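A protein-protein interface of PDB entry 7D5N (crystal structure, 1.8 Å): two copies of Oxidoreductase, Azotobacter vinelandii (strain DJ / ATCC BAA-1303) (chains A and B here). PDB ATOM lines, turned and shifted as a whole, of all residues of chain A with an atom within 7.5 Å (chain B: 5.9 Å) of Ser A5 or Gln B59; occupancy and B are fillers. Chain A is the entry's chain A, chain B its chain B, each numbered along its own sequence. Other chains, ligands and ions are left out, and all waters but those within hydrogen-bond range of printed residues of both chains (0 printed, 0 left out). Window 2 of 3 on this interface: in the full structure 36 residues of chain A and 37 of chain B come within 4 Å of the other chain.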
ATOM      1  N   ILE A   2      18.273 -30.182  13.450  1.00  0.00           N
ATOM      2  CA  ILE A   2      17.727 -29.654  12.174  1.00  0.00           C
ATOM      3  C   ILE A   2      18.010 -28.153  12.124  1.00  0.00           C
ATOM      4  O   ILE A   2      17.659 -27.449  13.089  1.00  0.00           O
ATOM      5  CB  ILE A   2      16.227 -29.964  11.973  1.00  0.00           C
ATOM      6  CG1 ILE A   2      16.004 -31.432  11.617  1.00  0.00           C
ATOM      7  CG2 ILE A   2      15.617 -29.059  10.911  1.00  0.00           C
ATOM      8  CD1 ILE A   2      14.552 -31.840  11.518  1.00  0.00           C
ATOM      9  N   ASN A   3      18.608 -27.675  11.029  1.00  0.00           N
ATOM     10  CA  ASN A   3      19.015 -26.252  10.909  1.00  0.00           C
ATOM     11  C   ASN A   3      18.589 -25.700   9.544  1.00  0.00           C
ATOM     12  O   ASN A   3      18.995 -24.578   9.233  1.00  0.00           O
ATOM     13  CB  ASN A   3      20.501 -26.088  11.244  1.00  0.00           C
ATOM     14  CG  ASN A   3      21.407 -26.787  10.254  1.00  0.00           C
ATOM     15  OD1 ASN A   3      20.950 -27.227   9.201  1.00  0.00           O
ATOM     16  ND2 ASN A   3      22.679 -26.895  10.598  1.00  0.00           N
ATOM     17  N   GLY A   4      17.720 -26.414   8.821  1.00  0.00           N
ATOM     18  CA  GLY A   4      17.154 -25.984   7.529  1.00  0.00           C
ATOM     19  C   GLY A   4      18.006 -26.398   6.350  1.00  0.00           C
ATOM     20  O   GLY A   4      17.666 -26.022   5.217  1.00  0.00           O
ATOM     21  N   SER A   5      19.099 -27.115   6.603  1.00  0.00           N
ATOM     22  CA  SER A   5      19.915 -27.748   5.547  1.00  0.00           C
ATOM     23  C   SER A   5      18.993 -28.598   4.687  1.00  0.00           C
ATOM     24  O   SER A   5      18.117 -29.309   5.174  1.00  0.00           O
ATOM     25  CB  SER A   5      21.027 -28.576   6.113  1.00  0.00           C
ATOM     26  OG  SER A   5      21.980 -27.738   6.739  1.00  0.00           O
ATOM     27  N   LYS A   6      19.243 -28.603   3.393  1.00  0.00           N
ATOM     28  CA  LYS A   6      18.499 -29.251   2.284  1.00  0.00           C
ATOM     29  C   LYS A   6      18.686 -30.771   2.437  1.00  0.00           C
ATOM     30  O   LYS A   6      19.782 -31.195   2.835  1.00  0.00           O
ATOM     31  CB  LYS A   6      19.134 -28.751   0.992  1.00  0.00           C
ATOM     32  CG  LYS A   6      20.458 -29.424   0.652  1.00  0.00           C
ATOM     33  CD  LYS A   6      21.160 -28.735  -0.472  1.00  0.00           C
ATOM     34  CE  LYS A   6      20.180 -28.244  -1.515  1.00  0.00           C
ATOM     35  NZ  LYS A   6      20.845 -27.379  -2.513  1.00  0.00           N
ATOM     36  N   ARG A   7      17.627 -31.576   2.380  1.00  0.00           N
ATOM     37  CA  ARG A   7      17.745 -33.049   2.528  1.00  0.00           C
ATOM     38  C   ARG A   7      17.935 -33.653   1.150  1.00  0.00           C
ATOM     39  O   ARG A   7      18.525 -34.742   1.041  1.00  0.00           O
ATOM     40  CB  ARG A   7      16.460 -33.625   3.109  1.00  0.00           C
ATOM     41  CG  ARG A   7      16.056 -32.972   4.414  1.00  0.00           C
ATOM     42  CD  ARG A   7      16.975 -33.514   5.464  1.00  0.00           C
ATOM     43  NE  ARG A   7      16.437 -33.143   6.747  1.00  0.00           N
ATOM     44  CZ  ARG A   7      16.603 -33.834   7.861  1.00  0.00           C
ATOM     45  NH1 ARG A   7      17.291 -34.971   7.862  1.00  0.00           N
ATOM     46  NH2 ARG A   7      16.055 -33.377   8.964  1.00  0.00           N
ATOM     47  N   ILE A   8      17.380 -32.970   0.154  1.00  0.00           N
ATOM     48  CA  ILE A   8      17.356 -33.454  -1.250  1.00  0.00           C
ATOM     49  C   ILE A   8      17.844 -32.302  -2.132  1.00  0.00           C
ATOM     50  O   ILE A   8      17.848 -31.150  -1.665  1.00  0.00           O
ATOM     51  CB  ILE A   8      15.958 -33.989  -1.627  1.00  0.00           C
ATOM     52  CG1 ILE A   8      14.885 -32.896  -1.564  1.00  0.00           C
ATOM     53  CG2 ILE A   8      15.580 -35.201  -0.772  1.00  0.00           C
ATOM     54  CD1 ILE A   8      13.551 -33.364  -2.093  1.00  0.00           C
ATOM     55  N   ASP A  36      12.007 -26.138   4.889  1.00  0.00           N
ATOM     56  CA  ASP A  36      13.368 -26.719   4.731  1.00  0.00           C
ATOM     57  C   ASP A  36      13.567 -27.237   3.297  1.00  0.00           C
ATOM     58  O   ASP A  36      14.323 -28.213   3.129  1.00  0.00           O
ATOM     59  CB  ASP A  36      13.577 -27.835   5.752  1.00  0.00           C
ATOM     60  CG  ASP A  36      13.271 -27.423   7.181  1.00  0.00           C
ATOM     61  OD1 ASP A  36      13.555 -26.248   7.546  1.00  0.00           O
ATOM     62  OD2 ASP A  36      12.732 -28.273   7.911  1.00  0.00           O
ATOM     63  N   GLN A  37      12.864 -26.653   2.324  1.00  0.00           N
ATOM     64  CA  GLN A  37      13.045 -26.900   0.865  1.00  0.00           C
ATOM     65  C   GLN A  37      12.658 -28.343   0.481  1.00  0.00           C
ATOM     66  O   GLN A  37      13.214 -28.865  -0.485  1.00  0.00           O
ATOM     67  CB  GLN A  37      14.501 -26.627   0.473  1.00  0.00           C
ATOM     68  CG  GLN A  37      15.057 -25.295   0.975  1.00  0.00           C
ATOM     69  CD  GLN A  37      16.570 -25.261   0.924  1.00  0.00           C
ATOM     70  OE1 GLN A  37      17.178 -25.010  -0.119  1.00  0.00           O
ATOM     71  NE2 GLN A  37      17.218 -25.566   2.043  1.00  0.00           N
ATOM     72  N   SER A  38      11.726 -28.981   1.181  1.00  0.00           N
ATOM     73  CA  SER A  38      11.310 -30.378   0.873  1.00  0.00           C
ATOM     74  C   SER A  38      10.482 -30.406  -0.417  1.00  0.00           C
ATOM     75  O   SER A  38      10.761 -31.218  -1.321  1.00  0.00           O
ATOM     76  CB  SER A  38      10.549 -30.986   2.036  1.00  0.00           C
ATOM     77  OG  SER A  38      11.404 -31.147   3.156  1.00  0.00           O
ATOM     78  N   TYR A 338       9.566 -34.085   5.576  1.00  0.00           N
ATOM     79  CA  TYR A 338      10.942 -34.162   5.018  1.00  0.00           C
ATOM     80  C   TYR A 338      11.248 -35.630   4.690  1.00  0.00           C
ATOM     81  O   TYR A 338      11.956 -35.883   3.708  1.00  0.00           O
ATOM     82  CB  TYR A 338      12.017 -33.476   5.862  1.00  0.00           C
ATOM     83  CG  TYR A 338      12.622 -34.291   6.975  1.00  0.00           C
ATOM     84  CD1 TYR A 338      13.509 -35.318   6.689  1.00  0.00           C
ATOM     85  CD2 TYR A 338      12.353 -34.005   8.309  1.00  0.00           C
ATOM     86  CE1 TYR A 338      14.089 -36.079   7.691  1.00  0.00           C
ATOM     87  CE2 TYR A 338      12.923 -34.759   9.325  1.00  0.00           C
ATOM     88  CZ  TYR A 338      13.800 -35.791   9.018  1.00  0.00           C
ATOM     89  OH  TYR A 338      14.382 -36.518  10.017  1.00  0.00           O
ATOM     90  N   ARG B  21      25.654 -22.600  11.070  1.00  0.00           N
ATOM     91  CA  ARG B  21      25.408 -24.059  11.115  1.00  0.00           C
ATOM     92  C   ARG B  21      25.174 -24.524  12.558  1.00  0.00           C
ATOM     93  O   ARG B  21      24.268 -25.342  12.754  1.00  0.00           O
ATOM     94  CB  ARG B  21      26.601 -24.807  10.508  1.00  0.00           C
ATOM     95  CG  ARG B  21      26.475 -26.324  10.541  1.00  0.00           C
ATOM     96  CD  ARG B  21      27.729 -27.053  10.059  1.00  0.00           C
ATOM     97  NE  ARG B  21      28.057 -26.764   8.668  1.00  0.00           N
ATOM     98  CZ  ARG B  21      27.360 -27.183   7.614  1.00  0.00           C
ATOM     99  NH1 ARG B  21      26.271 -27.918   7.783  1.00  0.00           N
ATOM    100  NH2 ARG B  21      27.743 -26.849   6.389  1.00  0.00           N
ATOM    101  N   ARG B  54      29.775 -19.962   4.222  1.00  0.00           N
ATOM    102  CA  ARG B  54      29.502 -20.222   2.793  1.00  0.00           C
ATOM    103  C   ARG B  54      29.056 -21.677   2.608  1.00  0.00           C
ATOM    104  O   ARG B  54      28.106 -21.890   1.855  1.00  0.00           O
ATOM    105  CB  ARG B  54      30.741 -19.865   1.969  1.00  0.00           C
ATOM    106  CG  ARG B  54      30.492 -19.909   0.472  1.00  0.00           C
ATOM    107  CD  ARG B  54      31.730 -19.749  -0.390  1.00  0.00           C
ATOM    108  NE  ARG B  54      32.983 -19.722   0.344  1.00  0.00           N
ATOM    109  CZ  ARG B  54      33.721 -20.792   0.614  1.00  0.00           C
ATOM    110  NH1 ARG B  54      33.331 -21.991   0.214  1.00  0.00           N
ATOM    111  NH2 ARG B  54      34.858 -20.657   1.274  1.00  0.00           N
ATOM    112  N   GLU B  55      29.716 -22.652   3.230  1.00  0.00           N
ATOM    113  CA  GLU B  55      29.286 -24.069   3.081  1.00  0.00           C
ATOM    114  C   GLU B  55      27.855 -24.215   3.599  1.00  0.00           C
ATOM    115  O   GLU B  55      27.054 -24.912   2.964  1.00  0.00           O
ATOM    116  CB  GLU B  55      30.182 -25.029   3.851  1.00  0.00           C
ATOM    117  CG  GLU B  55      31.529 -25.214   3.192  1.00  0.00           C
ATOM    118  CD  GLU B  55      32.447 -26.131   3.971  1.00  0.00           C
ATOM    119  OE1 GLU B  55      31.999 -27.244   4.319  1.00  0.00           O
ATOM    120  OE2 GLU B  55      33.600 -25.724   4.239  1.00  0.00           O
ATOM    121  N   PHE B  56      27.544 -23.570   4.719  1.00  0.00           N
ATOM    122  CA  PHE B  56      26.191 -23.660   5.323  1.00  0.00           C
ATOM    123  C   PHE B  56      25.206 -22.925   4.411  1.00  0.00           C
ATOM    124  O   PHE B  56      24.115 -23.463   4.127  1.00  0.00           O
ATOM    125  CB  PHE B  56      26.187 -23.114   6.747  1.00  0.00           C
ATOM    126  CG  PHE B  56      24.858 -23.267   7.437  1.00  0.00           C
ATOM    127  CD1 PHE B  56      24.218 -24.499   7.479  1.00  0.00           C
ATOM    128  CD2 PHE B  56      24.244 -22.175   8.036  1.00  0.00           C
ATOM    129  CE1 PHE B  56      22.984 -24.631   8.106  1.00  0.00           C
ATOM    130  CE2 PHE B  56      23.017 -22.315   8.671  1.00  0.00           C
ATOM    131  CZ  PHE B  56      22.396 -23.542   8.708  1.00  0.00           C
ATOM    132  N   GLY B  57      25.594 -21.746   3.924  1.00  0.00           N
ATOM    133  CA  GLY B  57      24.741 -20.934   3.033  1.00  0.00           C
ATOM    134  C   GLY B  57      24.280 -21.734   1.833  1.00  0.00           C
ATOM    135  O   GLY B  57      23.098 -21.631   1.438  1.00  0.00           O
ATOM    136  N   VAL B  58      25.180 -22.533   1.267  1.00  0.00           N
ATOM    137  CA  VAL B  58      24.891 -23.345   0.053  1.00  0.00           C
ATOM    138  C   VAL B  58      23.855 -24.412   0.426  1.00  0.00           C
ATOM    139  O   VAL B  58      22.897 -24.605  -0.342  1.00  0.00           O
ATOM    140  CB  VAL B  58      26.193 -23.918  -0.546  1.00  0.00           C
ATOM    141  CG1 VAL B  58      25.953 -25.134  -1.431  1.00  0.00           C
ATOM    142  CG2 VAL B  58      26.924 -22.823  -1.303  1.00  0.00           C
ATOM    143  N   GLN B  59      23.982 -25.014   1.605  1.00  0.00           N
ATOM    144  CA  GLN B  59      22.991 -26.015   2.091  1.00  0.00           C
ATOM    145  C   GLN B  59      21.616 -25.355   2.297  1.00  0.00           C
ATOM    146  O   GLN B  59      20.595 -26.061   2.201  1.00  0.00           O
ATOM    147  CB  GLN B  59      23.477 -26.655   3.386  1.00  0.00           C
ATOM    148  CG  GLN B  59      24.764 -27.442   3.238  1.00  0.00           C
ATOM    149  CD  GLN B  59      25.053 -28.179   4.524  1.00  0.00           C
ATOM    150  OE1 GLN B  59      25.214 -27.577   5.589  1.00  0.00           O
ATOM    151  NE2 GLN B  59      25.067 -29.500   4.453  1.00  0.00           N
ATOM    152  N   LEU B  60      21.574 -24.055   2.583  1.00  0.00           N
ATOM    153  CA  LEU B  60      20.301 -23.310   2.770  1.00  0.00           C
ATOM    154  C   LEU B  60      19.729 -22.893   1.414  1.00  0.00           C
ATOM    155  O   LEU B  60      18.673 -22.225   1.396  1.00  0.00           O
ATOM    156  CB  LEU B  60      20.572 -22.084   3.643  1.00  0.00           C
ATOM    157  CG  LEU B  60      20.966 -22.385   5.087  1.00  0.00           C
ATOM    158  CD1 LEU B  60      21.243 -21.099   5.853  1.00  0.00           C
ATOM    159  CD2 LEU B  60      19.890 -23.203   5.781  1.00  0.00           C
ATOM    160  N   GLY B  61      20.417 -23.223   0.319  1.00  0.00           N
ATOM    161  CA  GLY B  61      19.951 -22.884  -1.040  1.00  0.00           C
ATOM    162  C   GLY B  61      20.332 -21.473  -1.440  1.00  0.00           C
ATOM    163  O   GLY B  61      19.743 -20.969  -2.405  1.00  0.00           O
ATOM    164  N   VAL B  62      21.279 -20.852  -0.731  1.00  0.00           N
ATOM    165  CA  VAL B  62      21.760 -19.477  -1.036  1.00  0.00           C
ATOM    166  C   VAL B  62      22.828 -19.570  -2.137  1.00  0.00           C
ATOM    167  O   VAL B  62      23.675 -20.484  -2.079  1.00  0.00           O
ATOM    168  CB  VAL B  62      22.289 -18.746   0.210  1.00  0.00           C
ATOM    169  CG1 VAL B  62      22.813 -17.352  -0.121  1.00  0.00           C
ATOM    170  CG2 VAL B  62      21.231 -18.664   1.301  1.00  0.00           C
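The side-chain hydroxyl (OG) of Ser A5 is in hydrogen-bond range of the side-chain amide oxygen (OE1) of Gln B59 (3.4 Å).
ND2 of Asn A3 is in hydrogen-bond range of O of Arg B21 (3.1 Å).
The backbone NH (N) of Lys A6 lies within hydrogen-bond range of the backbone carbonyl oxygen (O) of Gln B59, at 3.1 Å.
O of Gln B59 is in hydrogen-bond range of NE2 of Gln A37, 3.4 Å away.
Of the 11 printed residues of chain A, 5 touch a printed residue of chain B.
Of the 10 printed residues of chain B, 5 touch a printed residue of chain A.
Hydrophobic or aromatic side chains of chain B within 4 Å of the printed part of chain A: Phe B56 and Leu B60.
Among the printed residues, 10 pairs touch across the chains.
Among the printed residues, no Asp or Glu carboxylate lies within 4 Å of a Lys or Arg side-chain nitrogen of the other chain.
No position is printed for both chains.
Asn A3 touches Phe B56.
O of Asn A3 touches CD2 of Leu B60 (3.8 Å).
Leu B60 touches Gly A4 (CD2 to O, 3.6 Å).
Ser A5 touches Phe B56.
Leu B60 touches Gln A37.
Gly B61 touches Gln A37 (CA to OE1, 3.6 Å).
Of the printed residues of chain B, Asn A3 touches Arg B21 (3.1 Å), Phe B56 (3.4 Å) and Leu B60 (3.8 Å).
Of the printed residues of chain B, Gly A4 touches Leu B60.
Ser A5 touches just these residues of chain B: Phe B56 (3.5 Å) and Gln B59 (3.4 Å).
Printed residues of chain A within 4 Å of Phe B56: Asn A3 and Ser A5.
Gln B59 touches just these residues of chain A: Ser A5, Lys A6 and Gln A37.
Printed residues of chain A within 4 Å of Gly B61: Gln A37 (3.6 Å).
Val B62 touches none of the printed residues of chain A.
The nearest residue of chain B that does not touch Ser A5 is Leu B60 (4.1 Å).
The nearest printed residue of chain B that does not touch Gln A37 is Val B58 (5.7 Å).
The backbone carbonyl oxygen (O) of Gly A4 lies within hydrogen-bond range of the side-chain amide nitrogen (NE2) of Gln A37 (3.2 Å).
NH1 of Arg B21 lies within hydrogen-bond range of OE1 of Gln B59, 2.5 Å away.
OD1 of Asn A3 is in hydrogen-bond range of OG of Ser A5, at 2.7 Å.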
